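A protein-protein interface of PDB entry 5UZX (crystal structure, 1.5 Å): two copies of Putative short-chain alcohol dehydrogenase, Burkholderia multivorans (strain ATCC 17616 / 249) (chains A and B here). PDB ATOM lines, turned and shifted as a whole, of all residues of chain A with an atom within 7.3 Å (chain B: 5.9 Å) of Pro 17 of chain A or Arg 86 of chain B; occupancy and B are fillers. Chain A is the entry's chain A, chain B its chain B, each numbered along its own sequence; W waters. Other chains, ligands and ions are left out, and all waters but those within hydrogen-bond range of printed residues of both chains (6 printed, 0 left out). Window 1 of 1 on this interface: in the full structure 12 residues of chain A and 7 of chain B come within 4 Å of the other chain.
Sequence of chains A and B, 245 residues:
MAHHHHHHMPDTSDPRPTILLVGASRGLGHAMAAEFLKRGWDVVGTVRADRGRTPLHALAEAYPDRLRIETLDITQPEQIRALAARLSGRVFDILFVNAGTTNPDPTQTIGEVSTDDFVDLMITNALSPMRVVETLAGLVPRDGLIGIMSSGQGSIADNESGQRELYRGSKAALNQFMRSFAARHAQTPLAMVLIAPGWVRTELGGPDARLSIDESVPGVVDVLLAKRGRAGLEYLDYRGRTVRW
The side-chain carboxylate (OE2) of Glu 70 of chain B lies within salt-bridge range of the guanidinium group (NH1) of Arg 228 of chain A, 2.8 Å away.
O of Ala 85 of chain B lies within hydrogen-bond range of NE1 of Trp 41 of chain A, 3.0 Å away.
The guanidinium group of Arg 86 of chain B is in salt-bridge range of the side-chain carboxylate of Asp 93 of chain A, 2.8 Å away.
The backbone carbonyl oxygen (O) of Pro 15 of chain A sits at hydrogen-bond distance from the guanidinium group (NH1) of Arg 86 of chain B (3.4 Å).
The side-chain carboxylate (OD2) of Asp 93 of chain A is in salt-bridge range of the guanidinium group (NH2) of Arg 228 of chain A, at 2.9 Å.
The backbone carbonyl oxygen of Ala 85 of chain B lies within hydrogen-bond range of the side-chain hydroxyl of Ser 88 of chain B, 3.2 Å away.
N of Asp 93 of chain A is in hydrogen-bond range of O of Thr 18 of chain A.
The backbone carbonyl oxygen of Arg 16 of chain A sits at hydrogen-bond distance from the side-chain hydroxyl of Thr 18 of chain A, 3.3 Å away.
O of Trp 41 of chain A lies within hydrogen-bond range of NH2 of Arg 66 of chain A (2.7 Å).
The backbone carbonyl oxygen of Pro 17 of chain A lies within hydrogen-bond range of the backbone NH of Asp 42 of chain A.
O of Pro 15 of chain A touches CB of Ala 82 of chain B (3.3 Å).
Ala 82 of chain B touches Arg 16 of chain A.
Pro 17 of chain A touches Ala 82 of chain B (CD to O, 3.6 Å).
Ala 85 of chain B touches Pro 17 of chain A (CB to CG, 3.8 Å).
CG of Arg 86 of chain B touches CB of Pro 17 of chain A (3.6 Å).
Ala 85 of chain B touches Arg 39 of chain A.
Gly 40 of chain A touches Ala 85 of chain B (O to CB, 3.7 Å).
Leu 225 of chain A touches Ser 88 of chain B (CD1 to OG, 3.6 Å).
Ala 226 of chain A touches Gly 89 of chain B.
CD of Arg 86 of chain B touches NH2 of Arg 228 of chain A (3.5 Å).
Of the printed residues of chain B, Pro 15 of chain A touches Ala 82 and Arg 86.
Of the printed residues of chain B, Ala 226 of chain A touches Gly 89.
Of the printed residues of chain B, Arg 228 of chain A touches Glu 70 and Arg 86.
Printed residues of chain A within 4 Å of Ala 82 of chain B: Pro 15, Arg 16 and Pro 17.
Arg 86 of chain B touches just these residues of chain A: Pro 15, Pro 17, Asp 93 and Arg 228.
Printed residues of chain A within 4 Å of Gly 89 of chain B: Ala 226 (3.8 Å).
The nearest residue of chain B that does not touch Pro 17 of chain A is Leu 83 of chain B (5.5 Å).
The nearest printed residue of chain B that does not touch Arg 228 of chain A is Leu 87 of chain B (4.1 Å).
Of the 12 printed residues of chain B, 6 touch a printed residue of chain A.
Printed residues of chain B that touch a printed residue of chain A: Glu 70, Ala 82, Ala 85, Arg 86, Ser 88 and Gly 89.
Hydrophobic or aromatic side chains of chain B within 4 Å of the printed part of chain A: Ala 82 and Ala 85.
Of the 19 printed residues of chain A, 10 touch a printed residue of chain B.
Hydrophobic or aromatic side chains of chain A that line the printed part of chain B: Pro 17, Trp 41, Leu 225 and Ala 226.
Among the printed residues, 14 pairs touch across the chains.
Among the printed residues, Asp or Glu carboxylates within 4 Å of a Lys or Arg side-chain nitrogen of the other chain: Asp 93 of chain A with Arg 86 of chain B (2.8 Å) and Arg 228 of chain A with Glu 70 of chain B (2.8 Å).
No position is printed for both chains.
Of the 14 pairs that touch across the chains among the printed residues, none has its exchanged pair printed and touching as well.
Water W3 bridges O of Arg 39 of chain A (2.5 Å) and OG of Ser 88 of chain B (3.5 Å).
Water W6 lies within hydrogen-bond range of O of Arg 86 of chain B, O of Leu 225 of chain A and N of Gly 89 of chain B.
Water W1 lies within hydrogen-bond range of the side-chain hydroxyl (OG) of Ser 88 of chain B (2.7 Å) and the guanidinium group (NH1) of Arg 39 of chain A (3.2 Å).
Water W4 lies within hydrogen-bond range of the guanidinium group of Arg 90 of chain B, the side-chain carboxylate of Glu 70 of chain B and the guanidinium group of Arg 228 of chain A.
Water W2 bridges the guanidinium group of Arg 228 of chain A (3.0 Å) and the backbone carbonyl oxygen of Arg 86 of chain B (3.4 Å).
Water W5 bridges the backbone carbonyl oxygen (O) of Pro 15 of chain A (3.1 Å) and the guanidinium group (NH2) of Arg 86 of chain B (3.2 Å).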
ATOM      1  N   PRO A  15     -35.482   0.099  -0.032  1.00  0.00           N
ATOM      2  CA  PRO A  15     -34.183   0.777  -0.140  1.00  0.00           C
ATOM      3  C   PRO A  15     -33.007  -0.172   0.102  1.00  0.00           C
ATOM      4  O   PRO A  15     -32.466  -0.730  -0.856  1.00  0.00           O
ATOM      5  CB  PRO A  15     -34.253   1.846   0.957  1.00  0.00           C
ATOM      6  CG  PRO A  15     -35.247   1.327   1.940  1.00  0.00           C
ATOM      7  CD  PRO A  15     -36.251   0.544   1.143  1.00  0.00           C
ATOM      8  N   ARG A  16     -32.626  -0.348   1.366  1.00  0.00           N
ATOM      9  CA  ARG A  16     -31.539  -1.247   1.707  1.00  0.00           C
ATOM     10  C   ARG A  16     -31.912  -2.688   1.362  1.00  0.00           C
ATOM     11  O   ARG A  16     -33.082  -3.077   1.447  1.00  0.00           O
ATOM     12  CB  ARG A  16     -31.246  -1.168   3.202  1.00  0.00           C
ATOM     13  CG  ARG A  16     -30.006  -0.371   3.572  1.00  0.00           C
ATOM     14  CD  ARG A  16     -29.773  -0.443   5.074  1.00  0.00           C
ATOM     15  NE  ARG A  16     -30.706   0.404   5.808  1.00  0.00           N
ATOM     16  CZ  ARG A  16     -30.337   1.433   6.563  1.00  0.00           C
ATOM     17  NH1 ARG A  16     -29.051   1.727   6.698  1.00  0.00           N
ATOM     18  NH2 ARG A  16     -31.251   2.159   7.192  1.00  0.00           N
ATOM     19  N   PRO A  17     -30.932  -3.505   0.980  1.00  0.00           N
ATOM     20  CA  PRO A  17     -31.211  -4.933   0.778  1.00  0.00           C
ATOM     21  C   PRO A  17     -31.719  -5.562   2.066  1.00  0.00           C
ATOM     22  O   PRO A  17     -31.265  -5.228   3.160  1.00  0.00           O
ATOM     23  CB  PRO A  17     -29.847  -5.505   0.377  1.00  0.00           C
ATOM     24  CG  PRO A  17     -28.860  -4.549   0.947  1.00  0.00           C
ATOM     25  CD  PRO A  17     -29.502  -3.196   0.800  1.00  0.00           C
ATOM     26  N   THR A  18     -32.677  -6.473   1.925  1.00  0.00           N
ATOM     27  CA  THR A  18     -33.323  -7.110   3.063  1.00  0.00           C
ATOM     28  C   THR A  18     -33.264  -8.624   2.917  1.00  0.00           C
ATOM     29  O   THR A  18     -33.474  -9.164   1.825  1.00  0.00           O
ATOM     30  CB  THR A  18     -34.777  -6.627   3.213  1.00  0.00           C
ATOM     31  OG1 THR A  18     -34.802  -5.193   3.241  1.00  0.00           O
ATOM     32  CG2 THR A  18     -35.386  -7.134   4.504  1.00  0.00           C
ATOM     33  N   ILE A  19     -32.945  -9.300   4.016  1.00  0.00           N
ATOM     34  CA  ILE A  19     -33.007 -10.756   4.111  1.00  0.00           C
ATOM     35  C   ILE A  19     -34.215 -11.131   4.952  1.00  0.00           C
ATOM     36  O   ILE A  19     -34.449 -10.555   6.022  1.00  0.00           O
ATOM     37  CB  ILE A  19     -31.716 -11.360   4.690  1.00  0.00           C
ATOM     38  CG1 ILE A  19     -31.864 -12.869   4.921  1.00  0.00           C
ATOM     39  CG2 ILE A  19     -31.310 -10.664   5.997  1.00  0.00           C
ATOM     40  CD1 ILE A  19     -30.552 -13.555   5.253  1.00  0.00           C
ATOM     41  N   PHE A  36     -25.846  -9.706   9.532  1.00  0.00           N
ATOM     42  CA  PHE A  36     -26.362  -8.991   8.371  1.00  0.00           C
ATOM     43  C   PHE A  36     -26.568  -7.513   8.669  1.00  0.00           C
ATOM     44  O   PHE A  36     -26.298  -6.658   7.813  1.00  0.00           O
ATOM     45  CB  PHE A  36     -27.644  -9.648   7.865  1.00  0.00           C
ATOM     46  CG  PHE A  36     -27.407 -10.666   6.799  1.00  0.00           C
ATOM     47  CD1 PHE A  36     -27.175 -10.268   5.486  1.00  0.00           C
ATOM     48  CD2 PHE A  36     -27.394 -12.019   7.103  1.00  0.00           C
ATOM     49  CE1 PHE A  36     -26.940 -11.197   4.490  1.00  0.00           C
ATOM     50  CE2 PHE A  36     -27.165 -12.966   6.102  1.00  0.00           C
ATOM     51  CZ  PHE A  36     -26.939 -12.557   4.804  1.00  0.00           C
ATOM     52  N   ARG A  39     -23.482  -5.607   8.219  1.00  0.00           N
ATOM     53  CA  ARG A  39     -23.095  -5.433   6.824  1.00  0.00           C
ATOM     54  C   ARG A  39     -23.977  -4.435   6.075  1.00  0.00           C
ATOM     55  O   ARG A  39     -23.906  -4.364   4.844  1.00  0.00           O
ATOM     56  CB  ARG A  39     -23.117  -6.776   6.078  1.00  0.00           C
ATOM     57  CG  ARG A  39     -22.507  -7.977   6.817  1.00  0.00           C
ATOM     58  CD  ARG A  39     -21.003  -8.099   6.647  1.00  0.00           C
ATOM     59  NE  ARG A  39     -20.486  -9.306   7.296  1.00  0.00           N
ATOM     60  CZ  ARG A  39     -20.004 -10.367   6.653  1.00  0.00           C
ATOM     61  NH1 ARG A  39     -19.942 -10.388   5.328  1.00  0.00           N
ATOM     62  NH2 ARG A  39     -19.563 -11.412   7.338  1.00  0.00           N
ATOM     63  N   GLY A  40     -24.817  -3.681   6.775  1.00  0.00           N
ATOM     64  CA  GLY A  40     -25.642  -2.696   6.103  1.00  0.00           C
ATOM     65  C   GLY A  40     -26.907  -3.235   5.475  1.00  0.00           C
ATOM     66  O   GLY A  40     -27.513  -2.533   4.658  1.00  0.00           O
ATOM     67  N   TRP A  41     -27.312  -4.461   5.810  1.00  0.00           N
ATOM     68  CA  TRP A  41     -28.580  -5.026   5.374  1.00  0.00           C
ATOM     69  C   TRP A  41     -29.666  -4.789   6.421  1.00  0.00           C
ATOM     70  O   TRP A  41     -29.390  -4.578   7.605  1.00  0.00           O
ATOM     71  CB  TRP A  41     -28.436  -6.535   5.139  1.00  0.00           C
ATOM     72  CG  TRP A  41     -27.764  -6.873   3.829  1.00  0.00           C
ATOM     73  CD1 TRP A  41     -26.531  -6.476   3.415  1.00  0.00           C
ATOM     74  CD2 TRP A  41     -28.296  -7.690   2.777  1.00  0.00           C
ATOM     75  NE1 TRP A  41     -26.261  -6.987   2.173  1.00  0.00           N
ATOM     76  CE2 TRP A  41     -27.327  -7.738   1.758  1.00  0.00           C
ATOM     77  CE3 TRP A  41     -29.502  -8.386   2.601  1.00  0.00           C
ATOM     78  CZ2 TRP A  41     -27.528  -8.443   0.565  1.00  0.00           C
ATOM     79  CZ3 TRP A  41     -29.696  -9.099   1.417  1.00  0.00           C
ATOM     80  CH2 TRP A  41     -28.711  -9.119   0.418  1.00  0.00           C
ATOM     81  N   ASP A  42     -30.914  -4.801   5.960  1.00  0.00           N
ATOM     82  CA  ASP A  42     -32.076  -4.904   6.834  1.00  0.00           C
ATOM     83  C   ASP A  42     -32.478  -6.368   6.958  1.00  0.00           C
ATOM     84  O   ASP A  42     -32.150  -7.201   6.112  1.00  0.00           O
ATOM     85  CB  ASP A  42     -33.246  -4.095   6.272  1.00  0.00           C
ATOM     86  CG  ASP A  42     -33.097  -2.603   6.520  1.00  0.00           C
ATOM     87  OD1 ASP A  42     -32.112  -2.203   7.178  1.00  0.00           O
ATOM     88  OD2 ASP A  42     -33.964  -1.832   6.052  1.00  0.00           O
ATOM     89  N   VAL A  43     -33.172  -6.688   8.049  1.00  0.00           N
ATOM     90  CA  VAL A  43     -33.540  -8.066   8.361  1.00  0.00           C
ATOM     91  C   VAL A  43     -35.009  -8.104   8.760  1.00  0.00           C
ATOM     92  O   VAL A  43     -35.445  -7.318   9.606  1.00  0.00           O
ATOM     93  CB  VAL A  43     -32.668  -8.650   9.496  1.00  0.00           C
ATOM     94  CG1 VAL A  43     -33.132 -10.063   9.884  1.00  0.00           C
ATOM     95  CG2 VAL A  43     -31.195  -8.651   9.097  1.00  0.00           C
ATOM     96  N   ARG A  66     -34.215  -1.254  11.483  1.00  0.00           N
ATOM     97  CA  ARG A  66     -33.608  -2.133  10.501  1.00  0.00           C
ATOM     98  C   ARG A  66     -33.917  -3.603  10.705  1.00  0.00           C
ATOM     99  O   ARG A  66     -33.733  -4.388   9.770  1.00  0.00           O
ATOM    100  CB  ARG A  66     -32.086  -1.935  10.478  1.00  0.00           C
ATOM    101  CG  ARG A  66     -31.692  -0.499  10.186  1.00  0.00           C
ATOM    102  CD  ARG A  66     -30.203  -0.329  10.192  1.00  0.00           C
ATOM    103  NE  ARG A  66     -29.577  -1.374   9.399  1.00  0.00           N
ATOM    104  CZ  ARG A  66     -28.270  -1.583   9.341  1.00  0.00           C
ATOM    105  NH1 ARG A  66     -27.440  -0.808  10.026  1.00  0.00           N
ATOM    106  NH2 ARG A  66     -27.797  -2.568   8.594  1.00  0.00           N
ATOM    107  N   VAL A  91     -40.171  -7.391  -1.304  1.00  0.00           N
ATOM    108  CA  VAL A  91     -39.165  -8.086  -2.089  1.00  0.00           C
ATOM    109  C   VAL A  91     -37.942  -8.270  -1.203  1.00  0.00           C
ATOM    110  O   VAL A  91     -37.461  -7.308  -0.592  1.00  0.00           O
ATOM    111  CB  VAL A  91     -38.807  -7.292  -3.355  1.00  0.00           C
ATOM    112  CG1 VAL A  91     -37.713  -8.006  -4.129  1.00  0.00           C
ATOM    113  CG2 VAL A  91     -40.052  -7.070  -4.212  1.00  0.00           C
ATOM    114  N   PHE A  92     -37.463  -9.502  -1.105  1.00  0.00           N
ATOM    115  CA  PHE A  92     -36.301  -9.823  -0.294  1.00  0.00           C
ATOM    116  C   PHE A  92     -35.200 -10.338  -1.200  1.00  0.00           C
ATOM    117  O   PHE A  92     -35.418 -11.268  -1.983  1.00  0.00           O
ATOM    118  CB  PHE A  92     -36.655 -10.873   0.757  1.00  0.00           C
ATOM    119  CG  PHE A  92     -37.711 -10.419   1.711  1.00  0.00           C
ATOM    120  CD1 PHE A  92     -37.372  -9.652   2.809  1.00  0.00           C
ATOM    121  CD2 PHE A  92     -39.043 -10.731   1.497  1.00  0.00           C
ATOM    122  CE1 PHE A  92     -38.344  -9.203   3.687  1.00  0.00           C
ATOM    123  CE2 PHE A  92     -40.026 -10.277   2.367  1.00  0.00           C
ATOM    124  CZ  PHE A  92     -39.675  -9.516   3.465  1.00  0.00           C
ATOM    125  N   ASP A  93     -34.018  -9.737  -1.081  1.00  0.00           N
ATOM    126  CA  ASP A  93     -32.881 -10.186  -1.869  1.00  0.00           C
ATOM    127  C   ASP A  93     -32.466 -11.601  -1.490  1.00  0.00           C
ATOM    128  O   ASP A  93     -32.007 -12.362  -2.345  1.00  0.00           O
ATOM    129  CB  ASP A  93     -31.716  -9.217  -1.686  1.00  0.00           C
ATOM    130  CG  ASP A  93     -31.842  -7.983  -2.563  1.00  0.00           C
ATOM    131  OD1 ASP A  93     -32.851  -7.260  -2.439  1.00  0.00           O
ATOM    132  OD2 ASP A  93     -30.933  -7.746  -3.377  1.00  0.00           O
ATOM    133  N   ILE A  94     -32.628 -11.975  -0.218  1.00  0.00           N
ATOM    134  CA  ILE A  94     -32.277 -13.297   0.285  1.00  0.00           C
ATOM    135  C   ILE A  94     -33.435 -13.812   1.122  1.00  0.00           C
ATOM    136  O   ILE A  94     -33.993 -13.074   1.942  1.00  0.00           O
ATOM    137  CB  ILE A  94     -30.984 -13.263   1.124  1.00  0.00           C
ATOM    138  CG1 ILE A  94     -29.810 -12.744   0.295  1.00  0.00           C
ATOM    139  CG2 ILE A  94     -30.653 -14.647   1.662  1.00  0.00           C
ATOM    140  CD1 ILE A  94     -28.522 -12.580   1.097  1.00  0.00           C
ATOM    141  N   LEU A 225     -23.321 -13.771   0.858  1.00  0.00           N
ATOM    142  CA  LEU A 225     -23.135 -12.573   0.044  1.00  0.00           C
ATOM    143  C   LEU A 225     -22.342 -12.861  -1.227  1.00  0.00           C
ATOM    144  O   LEU A 225     -22.559 -12.202  -2.249  1.00  0.00           O
ATOM    145  CB  LEU A 225     -22.476 -11.464   0.869  1.00  0.00           C
ATOM    146  CG  LEU A 225     -23.401 -10.905   1.953  1.00  0.00           C
ATOM    147  CD1 LEU A 225     -22.657  -9.929   2.854  1.00  0.00           C
ATOM    148  CD2 LEU A 225     -24.616 -10.221   1.332  1.00  0.00           C
ATOM    149  N   ALA A 226     -21.426 -13.830  -1.183  1.00  0.00           N
ATOM    150  CA  ALA A 226     -20.658 -14.204  -2.365  1.00  0.00           C
ATOM    151  C   ALA A 226     -21.434 -15.120  -3.301  1.00  0.00           C
ATOM    152  O   ALA A 226     -21.129 -15.157  -4.500  1.00  0.00           O
ATOM    153  CB  ALA A 226     -19.354 -14.885  -1.946  1.00  0.00           C
ATOM    154  N   ARG A 228     -24.727 -14.745  -3.798  1.00  0.00           N
ATOM    155  CA  ARG A 228     -25.683 -13.878  -4.474  1.00  0.00           C
ATOM    156  C   ARG A 228     -25.160 -13.548  -5.866  1.00  0.00           C
ATOM    157  O   ARG A 228     -24.048 -13.032  -6.013  1.00  0.00           O
ATOM    158  CB  ARG A 228     -25.872 -12.600  -3.653  1.00  0.00           C
ATOM    159  CG  ARG A 228     -26.866 -11.617  -4.257  1.00  0.00           C
ATOM    160  CD  ARG A 228     -27.002 -10.329  -3.447  1.00  0.00           C
ATOM    161  NE  ARG A 228     -28.077  -9.506  -4.002  1.00  0.00           N
ATOM    162  CZ  ARG A 228     -27.921  -8.649  -5.006  1.00  0.00           C
ATOM    163  NH1 ARG A 228     -26.728  -8.472  -5.565  1.00  0.00           N
ATOM    164  NH2 ARG A 228     -28.967  -7.961  -5.457  1.00  0.00           N
ATOM    165  N   GLU B  70     -28.753  -4.604 -11.567  1.00  0.00           N
ATOM    166  CA  GLU B  70     -29.061  -4.058 -10.249  1.00  0.00           C
ATOM    167  C   GLU B  70     -29.736  -2.712 -10.466  1.00  0.00           C
ATOM    168  O   GLU B  70     -29.698  -2.152 -11.563  1.00  0.00           O
ATOM    169  CB  GLU B  70     -27.788  -3.881  -9.411  1.00  0.00           C
ATOM    170  CG  GLU B  70     -26.951  -5.154  -9.204  1.00  0.00           C
ATOM    171  CD  GLU B  70     -27.526  -6.133  -8.192  1.00  0.00           C
ATOM    172  OE1 GLU B  70     -28.524  -5.807  -7.508  1.00  0.00           O
ATOM    173  OE2 GLU B  70     -26.969  -7.252  -8.077  1.00  0.00           O
ATOM    174  N   THR B  71     -30.372  -2.181  -9.422  1.00  0.00           N
ATOM    175  CA  THR B  71     -31.087  -0.918  -9.518  1.00  0.00           C
ATOM    176  C   THR B  71     -30.314   0.194  -8.819  1.00  0.00           C
ATOM    177  O   THR B  71     -29.738  -0.014  -7.746  1.00  0.00           O
ATOM    178  CB  THR B  71     -32.489  -1.029  -8.920  1.00  0.00           C
ATOM    179  OG1 THR B  71     -32.399  -1.371  -7.533  1.00  0.00           O
ATOM    180  CG2 THR B  71     -33.284  -2.094  -9.646  1.00  0.00           C
ATOM    181  N   ARG B  81     -25.643   3.563  -1.276  1.00  0.00           N
ATOM    182  CA  ARG B  81     -25.264   2.735  -0.136  1.00  0.00           C
ATOM    183  C   ARG B  81     -25.908   1.359  -0.213  1.00  0.00           C
ATOM    184  O   ARG B  81     -25.285   0.353   0.151  1.00  0.00           O
ATOM    185  CB  ARG B  81     -25.663   3.428   1.167  1.00  0.00           C
ATOM    186  CG  ARG B  81     -24.968   4.759   1.395  1.00  0.00           C
ATOM    187  CD  ARG B  81     -25.172   5.259   2.819  1.00  0.00           C
ATOM    188  NE  ARG B  81     -26.554   5.650   3.089  1.00  0.00           N
ATOM    189  CZ  ARG B  81     -27.029   6.880   2.913  1.00  0.00           C
ATOM    190  NH1 ARG B  81     -26.234   7.838   2.458  1.00  0.00           N
ATOM    191  NH2 ARG B  81     -28.295   7.153   3.193  1.00  0.00           N
ATOM    192  N   ALA B  82     -27.161   1.294  -0.674  1.00  0.00           N
ATOM    193  CA  ALA B  82     -27.830   0.005  -0.802  1.00  0.00           C
ATOM    194  C   ALA B  82     -27.127  -0.888  -1.815  1.00  0.00           C
ATOM    195  O   ALA B  82     -26.969  -2.096  -1.576  1.00  0.00           O
ATOM    196  CB  ALA B  82     -29.303   0.209  -1.156  1.00  0.00           C
ATOM    197  N   LEU B  83     -26.695  -0.318  -2.949  1.00  0.00           N
ATOM    198  CA  LEU B  83     -25.922  -1.091  -3.913  1.00  0.00           C
ATOM    199  C   LEU B  83     -24.607  -1.570  -3.308  1.00  0.00           C
ATOM    200  O   LEU B  83     -24.205  -2.728  -3.497  1.00  0.00           O
ATOM    201  CB  LEU B  83     -25.667  -0.264  -5.167  1.00  0.00           C
ATOM    202  CG  LEU B  83     -24.997  -1.029  -6.310  1.00  0.00           C
ATOM    203  CD1 LEU B  83     -25.869  -2.200  -6.731  1.00  0.00           C
ATOM    204  CD2 LEU B  83     -24.740  -0.089  -7.493  1.00  0.00           C
ATOM    205  N   ALA B  84     -23.931  -0.700  -2.554  1.00  0.00           N
ATOM    206  CA  ALA B  84     -22.686  -1.102  -1.917  1.00  0.00           C
ATOM    207  C   ALA B  84     -22.910  -2.291  -0.998  1.00  0.00           C
ATOM    208  O   ALA B  84     -22.099  -3.223  -0.962  1.00  0.00           O
ATOM    209  CB  ALA B  84     -22.095   0.076  -1.149  1.00  0.00           C
ATOM    210  N   ALA B  85     -24.013  -2.282  -0.245  1.00  0.00           N
ATOM    211  CA  ALA B  85     -24.293  -3.399   0.645  1.00  0.00           C
ATOM    212  C   ALA B  85     -24.632  -4.668  -0.132  1.00  0.00           C
ATOM    213  O   ALA B  85     -24.238  -5.768   0.279  1.00  0.00           O
ATOM    214  CB  ALA B  85     -25.408  -3.045   1.630  1.00  0.00           C
ATOM    215  N   ARG B  86     -25.373  -4.537  -1.235  1.00  0.00           N
ATOM    216  CA  ARG B  86     -25.730  -5.708  -2.032  1.00  0.00           C
ATOM    217  C   ARG B  86     -24.500  -6.371  -2.625  1.00  0.00           C
ATOM    218  O   ARG B  86     -24.445  -7.606  -2.739  1.00  0.00           O
ATOM    219  CB  ARG B  86     -26.677  -5.306  -3.161  1.00  0.00           C
ATOM    220  CG  ARG B  86     -28.122  -5.282  -2.745  1.00  0.00           C
ATOM    221  CD  ARG B  86     -29.036  -4.847  -3.888  1.00  0.00           C
ATOM    222  NE  ARG B  86     -30.415  -5.037  -3.456  1.00  0.00           N
ATOM    223  CZ  ARG B  86     -31.194  -4.074  -2.982  1.00  0.00           C
ATOM    224  NH1 ARG B  86     -30.748  -2.826  -2.905  1.00  0.00           N
ATOM    225  NH2 ARG B  86     -32.422  -4.364  -2.586  1.00  0.00           N
ATOM    226  N   LEU B  87     -23.513  -5.566  -3.017  1.00  0.00           N
ATOM    227  CA  LEU B  87     -22.340  -6.033  -3.743  1.00  0.00           C
ATOM    228  C   LEU B  87     -21.129  -6.253  -2.848  1.00  0.00           C
ATOM    229  O   LEU B  87     -20.032  -6.482  -3.361  1.00  0.00           O
ATOM    230  CB  LEU B  87     -21.986  -5.042  -4.856  1.00  0.00           C
ATOM    231  CG  LEU B  87     -23.076  -4.783  -5.895  1.00  0.00           C
ATOM    232  CD1 LEU B  87     -22.582  -3.811  -6.977  1.00  0.00           C
ATOM    233  CD2 LEU B  87     -23.537  -6.084  -6.512  1.00  0.00           C
ATOM    234  N   SER B  88     -21.302  -6.216  -1.530  1.00  0.00           N
ATOM    235  CA  SER B  88     -20.145  -6.238  -0.641  1.00  0.00           C
ATOM    236  C   SER B  88     -19.377  -7.554  -0.696  1.00  0.00           C
ATOM    237  O   SER B  88     -18.210  -7.593  -0.289  1.00  0.00           O
ATOM    238  CB  SER B  88     -20.571  -5.910   0.783  1.00  0.00           C
ATOM    239  OG  SER B  88     -21.456  -6.892   1.280  1.00  0.00           O
ATOM    240  N   GLY B  89     -19.998  -8.621  -1.194  1.00  0.00           N
ATOM    241  CA  GLY B  89     -19.309  -9.880  -1.421  1.00  0.00           C
ATOM    242  C   GLY B  89     -18.775 -10.066  -2.833  1.00  0.00           C
ATOM    243  O   GLY B  89     -18.583 -11.206  -3.271  1.00  0.00           O
ATOM    244  N   ARG B  90     -18.523  -8.967  -3.553  1.00  0.00           N
ATOM    245  CA  ARG B  90     -18.027  -9.022  -4.925  1.00  0.00           C
ATOM    246  C   ARG B  90     -16.858  -8.063  -5.125  1.00  0.00           C
ATOM    247  O   ARG B  90     -16.741  -7.042  -4.444  1.00  0.00           O
ATOM    248  CB  ARG B  90     -19.123  -8.675  -5.952  1.00  0.00           C
ATOM    249  CG  ARG B  90     -20.197  -9.730  -6.080  1.00  0.00           C
ATOM    250  CD  ARG B  90     -21.110  -9.482  -7.273  1.00  0.00           C
ATOM    251  NE  ARG B  90     -20.482  -9.837  -8.544  1.00  0.00           N
ATOM    252  CZ  ARG B  90     -21.150 -10.282  -9.606  1.00  0.00           C
ATOM    253  NH1 ARG B  90     -22.469 -10.436  -9.549  1.00  0.00           N
ATOM    254  NH2 ARG B  90     -20.503 -10.587 -10.725  1.00  0.00           N
HETATM  255  O   HOH W   1     -19.892  -7.952   3.247  1.00  0.00           O
HETATM  256  O   HOH W   2     -24.039  -9.824  -5.263  1.00  0.00           O
HETATM  257  O   HOH W   3     -21.886  -4.240   3.448  1.00  0.00           O
HETATM  258  O   HOH W   4     -24.273  -8.781  -7.917  1.00  0.00           O
HETATM  259  O   HOH W   5     -33.661  -1.559  -3.585  1.00  0.00           O
HETATM  260  O   HOH W   6     -22.600  -9.424  -2.702  1.00  0.00           O
